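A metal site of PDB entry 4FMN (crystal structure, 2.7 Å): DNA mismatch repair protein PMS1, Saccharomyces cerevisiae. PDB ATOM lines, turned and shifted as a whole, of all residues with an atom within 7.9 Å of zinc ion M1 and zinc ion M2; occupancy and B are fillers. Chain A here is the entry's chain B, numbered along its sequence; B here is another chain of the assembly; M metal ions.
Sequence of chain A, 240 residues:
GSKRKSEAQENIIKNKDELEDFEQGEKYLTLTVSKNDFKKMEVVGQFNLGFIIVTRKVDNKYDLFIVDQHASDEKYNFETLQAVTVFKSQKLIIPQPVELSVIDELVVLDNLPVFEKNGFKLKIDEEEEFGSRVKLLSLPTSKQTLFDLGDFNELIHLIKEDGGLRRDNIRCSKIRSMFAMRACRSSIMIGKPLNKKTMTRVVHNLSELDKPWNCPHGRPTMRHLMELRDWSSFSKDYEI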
ATOM      1  N   ASP A  68     -29.932 -14.278   9.211  1.00  0.00           N
ATOM      2  CA  ASP A  68     -29.883 -15.380   8.246  1.00  0.00           C
ATOM      3  C   ASP A  68     -31.244 -16.099   8.353  1.00  0.00           C
ATOM      4  O   ASP A  68     -31.554 -16.659   9.421  1.00  0.00           O
ATOM      5  CB  ASP A  68     -28.731 -16.336   8.611  1.00  0.00           C
ATOM      6  CG  ASP A  68     -28.436 -17.445   7.606  1.00  0.00           C
ATOM      7  OD1 ASP A  68     -29.359 -18.284   7.337  1.00  0.00           O
ATOM      8  OD2 ASP A  68     -27.271 -17.507   7.103  1.00  0.00           O
ATOM      9  N   HIS A  70     -32.435 -18.934   7.126  1.00  0.00           N
ATOM     10  CA  HIS A  70     -32.367 -20.373   7.406  1.00  0.00           C
ATOM     11  C   HIS A  70     -31.931 -20.672   8.842  1.00  0.00           C
ATOM     12  O   HIS A  70     -32.677 -21.334   9.556  1.00  0.00           O
ATOM     13  CB  HIS A  70     -31.504 -21.137   6.375  1.00  0.00           C
ATOM     14  CG  HIS A  70     -31.282 -22.573   6.709  1.00  0.00           C
ATOM     15  ND1 HIS A  70     -32.286 -23.520   6.554  1.00  0.00           N
ATOM     16  CD2 HIS A  70     -30.184 -23.193   7.224  1.00  0.00           C
ATOM     17  CE1 HIS A  70     -31.781 -24.678   6.974  1.00  0.00           C
ATOM     18  NE2 HIS A  70     -30.524 -24.530   7.390  1.00  0.00           N
ATOM     19  N   ALA A  71     -30.750 -20.190   9.256  1.00  0.00           N
ATOM     20  CA  ALA A  71     -30.158 -20.445  10.581  1.00  0.00           C
ATOM     21  C   ALA A  71     -31.033 -19.983  11.749  1.00  0.00           C
ATOM     22  O   ALA A  71     -31.153 -20.686  12.742  1.00  0.00           O
ATOM     23  CB  ALA A  71     -28.758 -19.842  10.668  1.00  0.00           C
ATOM     24  N   SER A  72     -31.709 -18.851  11.588  1.00  0.00           N
ATOM     25  CA  SER A  72     -32.621 -18.342  12.628  1.00  0.00           C
ATOM     26  C   SER A  72     -33.898 -19.175  12.705  1.00  0.00           C
ATOM     27  O   SER A  72     -34.381 -19.480  13.803  1.00  0.00           O
ATOM     28  CB  SER A  72     -32.946 -16.877  12.391  1.00  0.00           C
ATOM     29  OG  SER A  72     -33.511 -16.740  11.104  1.00  0.00           O
ATOM     30  N   GLU A  74     -34.172 -22.345  11.809  1.00  0.00           N
ATOM     31  CA  GLU A  74     -33.615 -23.608  12.276  1.00  0.00           C
ATOM     32  C   GLU A  74     -33.386 -23.605  13.777  1.00  0.00           C
ATOM     33  O   GLU A  74     -33.795 -24.567  14.425  1.00  0.00           O
ATOM     34  CB  GLU A  74     -32.302 -23.908  11.502  1.00  0.00           C
ATOM     35  CG  GLU A  74     -31.674 -25.235  11.866  1.00  0.00           C
ATOM     36  CD  GLU A  74     -30.384 -25.467  11.131  1.00  0.00           C
ATOM     37  OE1 GLU A  74     -30.419 -25.632   9.892  1.00  0.00           O
ATOM     38  OE2 GLU A  74     -29.324 -25.437  11.800  1.00  0.00           O
ATOM     39  N   LYS A  75     -32.727 -22.559  14.346  1.00  0.00           N
ATOM     40  CA  LYS A  75     -32.478 -22.504  15.804  1.00  0.00           C
ATOM     41  C   LYS A  75     -33.803 -22.597  16.566  1.00  0.00           C
ATOM     42  O   LYS A  75     -33.863 -23.254  17.608  1.00  0.00           O
ATOM     43  CB  LYS A  75     -31.675 -21.243  16.194  1.00  0.00           C
ATOM     44  CG  LYS A  75     -31.373 -21.063  17.700  1.00  0.00           C
ATOM     45  CD  LYS A  75     -30.677 -22.273  18.323  1.00  0.00           C
ATOM     46  CE  LYS A  75     -29.976 -21.945  19.621  1.00  0.00           C
ATOM     47  NZ  LYS A  75     -28.950 -22.983  19.956  1.00  0.00           N
ATOM     48  N   PHE A  78     -35.274 -26.340  16.039  1.00  0.00           N
ATOM     49  CA  PHE A  78     -34.372 -27.189  16.788  1.00  0.00           C
ATOM     50  C   PHE A  78     -34.685 -27.127  18.289  1.00  0.00           C
ATOM     51  O   PHE A  78     -34.876 -28.178  18.913  1.00  0.00           O
ATOM     52  CB  PHE A  78     -32.892 -26.820  16.525  1.00  0.00           C
ATOM     53  CG  PHE A  78     -31.897 -27.480  17.456  1.00  0.00           C
ATOM     54  CD1 PHE A  78     -31.560 -28.824  17.313  1.00  0.00           C
ATOM     55  CD2 PHE A  78     -31.302 -26.760  18.489  1.00  0.00           C
ATOM     56  CE1 PHE A  78     -30.659 -29.442  18.184  1.00  0.00           C
ATOM     57  CE2 PHE A  78     -30.402 -27.378  19.361  1.00  0.00           C
ATOM     58  CZ  PHE A  78     -30.083 -28.714  19.203  1.00  0.00           C
ATOM     59  N   ALA A 180     -31.050 -31.832  14.947  1.00  0.00           N
ATOM     60  CA  ALA A 180     -30.338 -30.812  14.179  1.00  0.00           C
ATOM     61  C   ALA A 180     -30.596 -31.039  12.688  1.00  0.00           C
ATOM     62  O   ALA A 180     -30.817 -30.086  11.971  1.00  0.00           O
ATOM     63  CB  ALA A 180     -28.855 -30.854  14.496  1.00  0.00           C
ATOM     64  N   MET A 181     -30.662 -32.301  12.235  1.00  0.00           N
ATOM     65  CA  MET A 181     -30.960 -32.592  10.840  1.00  0.00           C
ATOM     66  C   MET A 181     -32.441 -32.389  10.537  1.00  0.00           C
ATOM     67  O   MET A 181     -32.759 -31.857   9.476  1.00  0.00           O
ATOM     68  CB  MET A 181     -30.498 -33.995  10.440  1.00  0.00           C
ATOM     69  CG  MET A 181     -30.144 -34.094   8.978  1.00  0.00           C
ATOM     70  SD  MET A 181     -29.476 -35.730   8.576  1.00  0.00           S
ATOM     71  CE  MET A 181     -29.274 -35.532   6.797  1.00  0.00           C
ATOM     72  N   ALA A 183     -34.487 -30.238  11.960  1.00  0.00           N
ATOM     73  CA  ALA A 183     -34.635 -28.786  11.931  1.00  0.00           C
ATOM     74  C   ALA A 183     -34.082 -28.223  10.618  1.00  0.00           C
ATOM     75  O   ALA A 183     -34.775 -27.455   9.957  1.00  0.00           O
ATOM     76  CB  ALA A 183     -33.919 -28.165  13.124  1.00  0.00           C
ATOM     77  N   CYS A 184     -32.881 -28.634  10.223  1.00  0.00           N
ATOM     78  CA  CYS A 184     -32.252 -28.165   8.990  1.00  0.00           C
ATOM     79  C   CYS A 184     -33.075 -28.454   7.721  1.00  0.00           C
ATOM     80  O   CYS A 184     -33.173 -27.600   6.836  1.00  0.00           O
ATOM     81  CB  CYS A 184     -30.831 -28.705   8.876  1.00  0.00           C
ATOM     82  SG  CYS A 184     -29.932 -28.100   7.437  1.00  0.00           S
ATOM     83  N   ARG A 185     -33.684 -29.636   7.648  1.00  0.00           N
ATOM     84  CA  ARG A 185     -34.489 -30.064   6.517  1.00  0.00           C
ATOM     85  C   ARG A 185     -35.883 -29.431   6.486  1.00  0.00           C
ATOM     86  O   ARG A 185     -36.435 -29.232   5.419  1.00  0.00           O
ATOM     87  CB  ARG A 185     -34.561 -31.607   6.448  1.00  0.00           C
ATOM     88  CG  ARG A 185     -33.192 -32.253   6.241  1.00  0.00           C
ATOM     89  CD  ARG A 185     -33.264 -33.706   5.808  1.00  0.00           C
ATOM     90  NE  ARG A 185     -33.258 -33.838   4.343  1.00  0.00           N
ATOM     91  CZ  ARG A 185     -32.239 -34.316   3.636  1.00  0.00           C
ATOM     92  NH1 ARG A 185     -31.134 -34.724   4.238  1.00  0.00           N
ATOM     93  NH2 ARG A 185     -32.331 -34.396   2.309  1.00  0.00           N
ATOM     94  N   SER A 186     -36.464 -29.112   7.644  1.00  0.00           N
ATOM     95  CA  SER A 186     -37.802 -28.554   7.701  1.00  0.00           C
ATOM     96  C   SER A 186     -37.871 -27.014   7.721  1.00  0.00           C
ATOM     97  O   SER A 186     -38.928 -26.440   7.495  1.00  0.00           O
ATOM     98  CB  SER A 186     -38.558 -29.136   8.893  1.00  0.00           C
ATOM     99  OG  SER A 186     -38.077 -28.627  10.125  1.00  0.00           O
ATOM    100  N   SER A 187     -36.730 -26.355   8.003  1.00  0.00           N
ATOM    101  CA  SER A 187     -36.645 -24.910   8.082  1.00  0.00           C
ATOM    102  C   SER A 187     -36.664 -24.210   6.713  1.00  0.00           C
ATOM    103  O   SER A 187     -36.571 -24.866   5.668  1.00  0.00           O
ATOM    104  CB  SER A 187     -35.412 -24.513   8.880  1.00  0.00           C
ATOM    105  OG  SER A 187     -35.564 -24.998  10.203  1.00  0.00           O
ATOM    106  N   ILE A 188     -36.821 -22.879   6.737  1.00  0.00           N
ATOM    107  CA  ILE A 188     -36.852 -22.020   5.552  1.00  0.00           C
ATOM    108  C   ILE A 188     -35.516 -22.177   4.838  1.00  0.00           C
ATOM    109  O   ILE A 188     -34.459 -22.117   5.485  1.00  0.00           O
ATOM    110  CB  ILE A 188     -37.163 -20.532   5.939  1.00  0.00           C
ATOM    111  CG1 ILE A 188     -38.636 -20.368   6.232  1.00  0.00           C
ATOM    112  CG2 ILE A 188     -36.708 -19.476   4.886  1.00  0.00           C
ATOM    113  CD1 ILE A 188     -38.913 -19.288   7.196  1.00  0.00           C
ATOM    114  N   ASN A 214     -26.553 -18.704  17.535  1.00  0.00           N
ATOM    115  CA  ASN A 214     -26.099 -19.737  16.612  1.00  0.00           C
ATOM    116  C   ASN A 214     -27.110 -20.816  16.389  1.00  0.00           C
ATOM    117  O   ASN A 214     -27.869 -21.127  17.301  1.00  0.00           O
ATOM    118  CB  ASN A 214     -24.793 -20.398  17.095  1.00  0.00           C
ATOM    119  CG  ASN A 214     -23.640 -19.447  17.164  1.00  0.00           C
ATOM    120  OD1 ASN A 214     -23.148 -18.950  16.152  1.00  0.00           O
ATOM    121  ND2 ASN A 214     -23.204 -19.174  18.392  1.00  0.00           N
ATOM    122  N   CYS A 215     -27.069 -21.447  15.202  1.00  0.00           N
ATOM    123  CA  CYS A 215     -27.918 -22.571  14.836  1.00  0.00           C
ATOM    124  C   CYS A 215     -27.284 -23.817  15.510  1.00  0.00           C
ATOM    125  O   CYS A 215     -26.126 -23.738  15.960  1.00  0.00           O
ATOM    126  CB  CYS A 215     -27.948 -22.706  13.311  1.00  0.00           C
ATOM    127  SG  CYS A 215     -26.609 -23.726  12.620  1.00  0.00           S
ATOM    128  N   PRO A 216     -27.948 -24.993  15.514  1.00  0.00           N
ATOM    129  CA  PRO A 216     -27.311 -26.189  16.129  1.00  0.00           C
ATOM    130  C   PRO A 216     -25.967 -26.646  15.522  1.00  0.00           C
ATOM    131  O   PRO A 216     -25.242 -27.401  16.158  1.00  0.00           O
ATOM    132  CB  PRO A 216     -28.379 -27.263  16.028  1.00  0.00           C
ATOM    133  CG  PRO A 216     -29.324 -26.780  14.975  1.00  0.00           C
ATOM    134  CD  PRO A 216     -29.318 -25.303  15.053  1.00  0.00           C
ATOM    135  N   HIS A 217     -25.626 -26.184  14.304  1.00  0.00           N
ATOM    136  CA  HIS A 217     -24.357 -26.548  13.670  1.00  0.00           C
ATOM    137  C   HIS A 217     -23.256 -25.531  13.988  1.00  0.00           C
ATOM    138  O   HIS A 217     -22.115 -25.746  13.598  1.00  0.00           O
ATOM    139  CB  HIS A 217     -24.530 -26.706  12.163  1.00  0.00           C
ATOM    140  CG  HIS A 217     -25.669 -27.577  11.813  1.00  0.00           C
ATOM    141  ND1 HIS A 217     -26.921 -27.031  11.583  1.00  0.00           N
ATOM    142  CD2 HIS A 217     -25.741 -28.929  11.735  1.00  0.00           C
ATOM    143  CE1 HIS A 217     -27.714 -28.069  11.343  1.00  0.00           C
ATOM    144  NE2 HIS A 217     -27.024 -29.230  11.401  1.00  0.00           N
ATOM    145  N   GLY A 218     -23.607 -24.448  14.679  1.00  0.00           N
ATOM    146  CA  GLY A 218     -22.667 -23.406  15.086  1.00  0.00           C
ATOM    147  C   GLY A 218     -22.558 -22.201  14.175  1.00  0.00           C
ATOM    148  O   GLY A 218     -21.629 -21.401  14.324  1.00  0.00           O
ATOM    149  N   ARG A 219     -23.484 -22.068  13.215  1.00  0.00           N
ATOM    150  CA  ARG A 219     -23.510 -20.967  12.246  1.00  0.00           C
ATOM    151  C   ARG A 219     -24.282 -19.793  12.841  1.00  0.00           C
ATOM    152  O   ARG A 219     -25.265 -20.014  13.529  1.00  0.00           O
ATOM    153  CB  ARG A 219     -24.186 -21.403  10.931  1.00  0.00           C
ATOM    154  CG  ARG A 219     -23.693 -22.693  10.350  1.00  0.00           C
ATOM    155  CD  ARG A 219     -22.222 -22.666  10.017  1.00  0.00           C
ATOM    156  NE  ARG A 219     -21.684 -24.022  10.061  1.00  0.00           N
ATOM    157  CZ  ARG A 219     -20.405 -24.324  10.150  1.00  0.00           C
ATOM    158  NH1 ARG A 219     -19.494 -23.365  10.192  1.00  0.00           N
ATOM    159  NH2 ARG A 219     -20.026 -25.595  10.226  1.00  0.00           N
ATOM    160  N   PRO A 220     -23.886 -18.541  12.557  1.00  0.00           N
ATOM    161  CA  PRO A 220     -24.601 -17.412  13.173  1.00  0.00           C
ATOM    162  C   PRO A 220     -25.994 -17.211  12.615  1.00  0.00           C
ATOM    163  O   PRO A 220     -26.236 -17.466  11.435  1.00  0.00           O
ATOM    164  CB  PRO A 220     -23.663 -16.219  12.944  1.00  0.00           C
ATOM    165  CG  PRO A 220     -22.838 -16.585  11.836  1.00  0.00           C
ATOM    166  CD  PRO A 220     -22.723 -18.071  11.782  1.00  0.00           C
ATOM    167  N   GLU B 286     -22.597 -18.888   7.261  1.00  0.00           N
ATOM    168  CA  GLU B 286     -22.192 -20.066   6.474  1.00  0.00           C
ATOM    169  C   GLU B 286     -23.229 -21.177   6.514  1.00  0.00           C
ATOM    170  O   GLU B 286     -24.003 -21.259   7.466  1.00  0.00           O
ATOM    171  CB  GLU B 286     -20.827 -20.621   6.938  1.00  0.00           C
ATOM    172  CG  GLU B 286     -19.736 -19.605   7.260  1.00  0.00           C
ATOM    173  CD  GLU B 286     -18.333 -20.177   7.350  1.00  0.00           C
ATOM    174  OE1 GLU B 286     -18.122 -21.150   8.116  1.00  0.00           O
ATOM    175  OE2 GLU B 286     -17.444 -19.652   6.636  1.00  0.00           O
ATOM    176  N   ARG B 287     -23.207 -22.060   5.507  1.00  0.00           N
ATOM    177  CA  ARG B 287     -24.093 -23.198   5.409  1.00  0.00           C
ATOM    178  C   ARG B 287     -23.859 -24.159   6.588  1.00  0.00           C
ATOM    179  O   ARG B 287     -22.752 -24.256   7.111  1.00  0.00           O
ATOM    180  CB  ARG B 287     -23.918 -23.926   4.081  1.00  0.00           C
ATOM    181  CG  ARG B 287     -22.575 -24.664   3.921  1.00  0.00           C
ATOM    182  CD  ARG B 287     -22.275 -25.070   2.494  1.00  0.00           C
ATOM    183  NE  ARG B 287     -22.266 -23.915   1.595  1.00  0.00           N
ATOM    184  CZ  ARG B 287     -22.145 -24.016   0.276  1.00  0.00           C
ATOM    185  NH1 ARG B 287     -22.007 -25.209  -0.299  1.00  0.00           N
ATOM    186  NH2 ARG B 287     -22.178 -22.925  -0.483  1.00  0.00           N
ATOM    187  N   CYS B 288     -24.944 -24.842   6.990  1.00  0.00           N
ATOM    188  CA  CYS B 288     -24.942 -25.775   8.092  1.00  0.00           C
ATOM    189  C   CYS B 288     -24.077 -26.920   7.696  1.00  0.00           C
ATOM    190  O   CYS B 288     -24.323 -27.426   6.581  1.00  0.00           O
ATOM    191  CB  CYS B 288     -26.369 -26.219   8.412  1.00  0.00           C
ATOM    192  SG  CYS B 288     -27.480 -24.866   8.840  1.00  0.00           S
ATOM    193  OXT CYS B 288     -23.067 -27.146   8.374  1.00  0.00           O
HETATM  194 ZN    ZN M   1     -27.521 -25.260  11.103  1.00  0.00          ZN
HETATM  195 ZN    ZN M   2     -29.406 -25.931   8.343  1.00  0.00          ZN
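Zinc ion M2 is bound by the side-chain carboxylate of Glu 74 (1.9 Å), a ring nitrogen (NE2) of His 70 (2.0 Å), the side-chain sulfur of Cys 288 of chain B (2.3 Å) and the side-chain sulfur of Cys 184 (2.4 Å).
The chain-end carboxylate (OXT) of Cys 288 of chain B lies within salt-bridge range of the guanidinium group (NE) of Arg 219. OD1 of Asp 68 sits at hydrogen-bond distance from N of His 70 (3.2 Å). The backbone NH (N) of Gly 218 sits close to the side-chain sulfur (SG) of Cys 215. SG of Cys 215 lies close to N of Arg 219, at 3.6 Å. ND1 of His 70 is in hydrogen-bond range of O of Ile 188. The backbone NH (N) of Glu 74 lies close to the side-chain hydroxyl (OG) of Ser 187.
Of the 25 residues printed, 4 come within 4 Å of zinc ion M2. The nearest printed residue that does not touch zinc ion M2 is His 217 (4.1 Å).
Of the 25 residues printed, 4 come within 4 Å of zinc ion M1.
Zinc ion M1 is bound by a ring nitrogen (ND1) of His 217 (1.9 Å), the side-chain carboxylate of Glu 74 (1.9 Å), the side-chain sulfur of Cys 288 of chain B (2.3 Å) and the side-chain sulfur of Cys 215 (2.3 Å). Zinc ion M1 has four donor atoms within binding distance.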
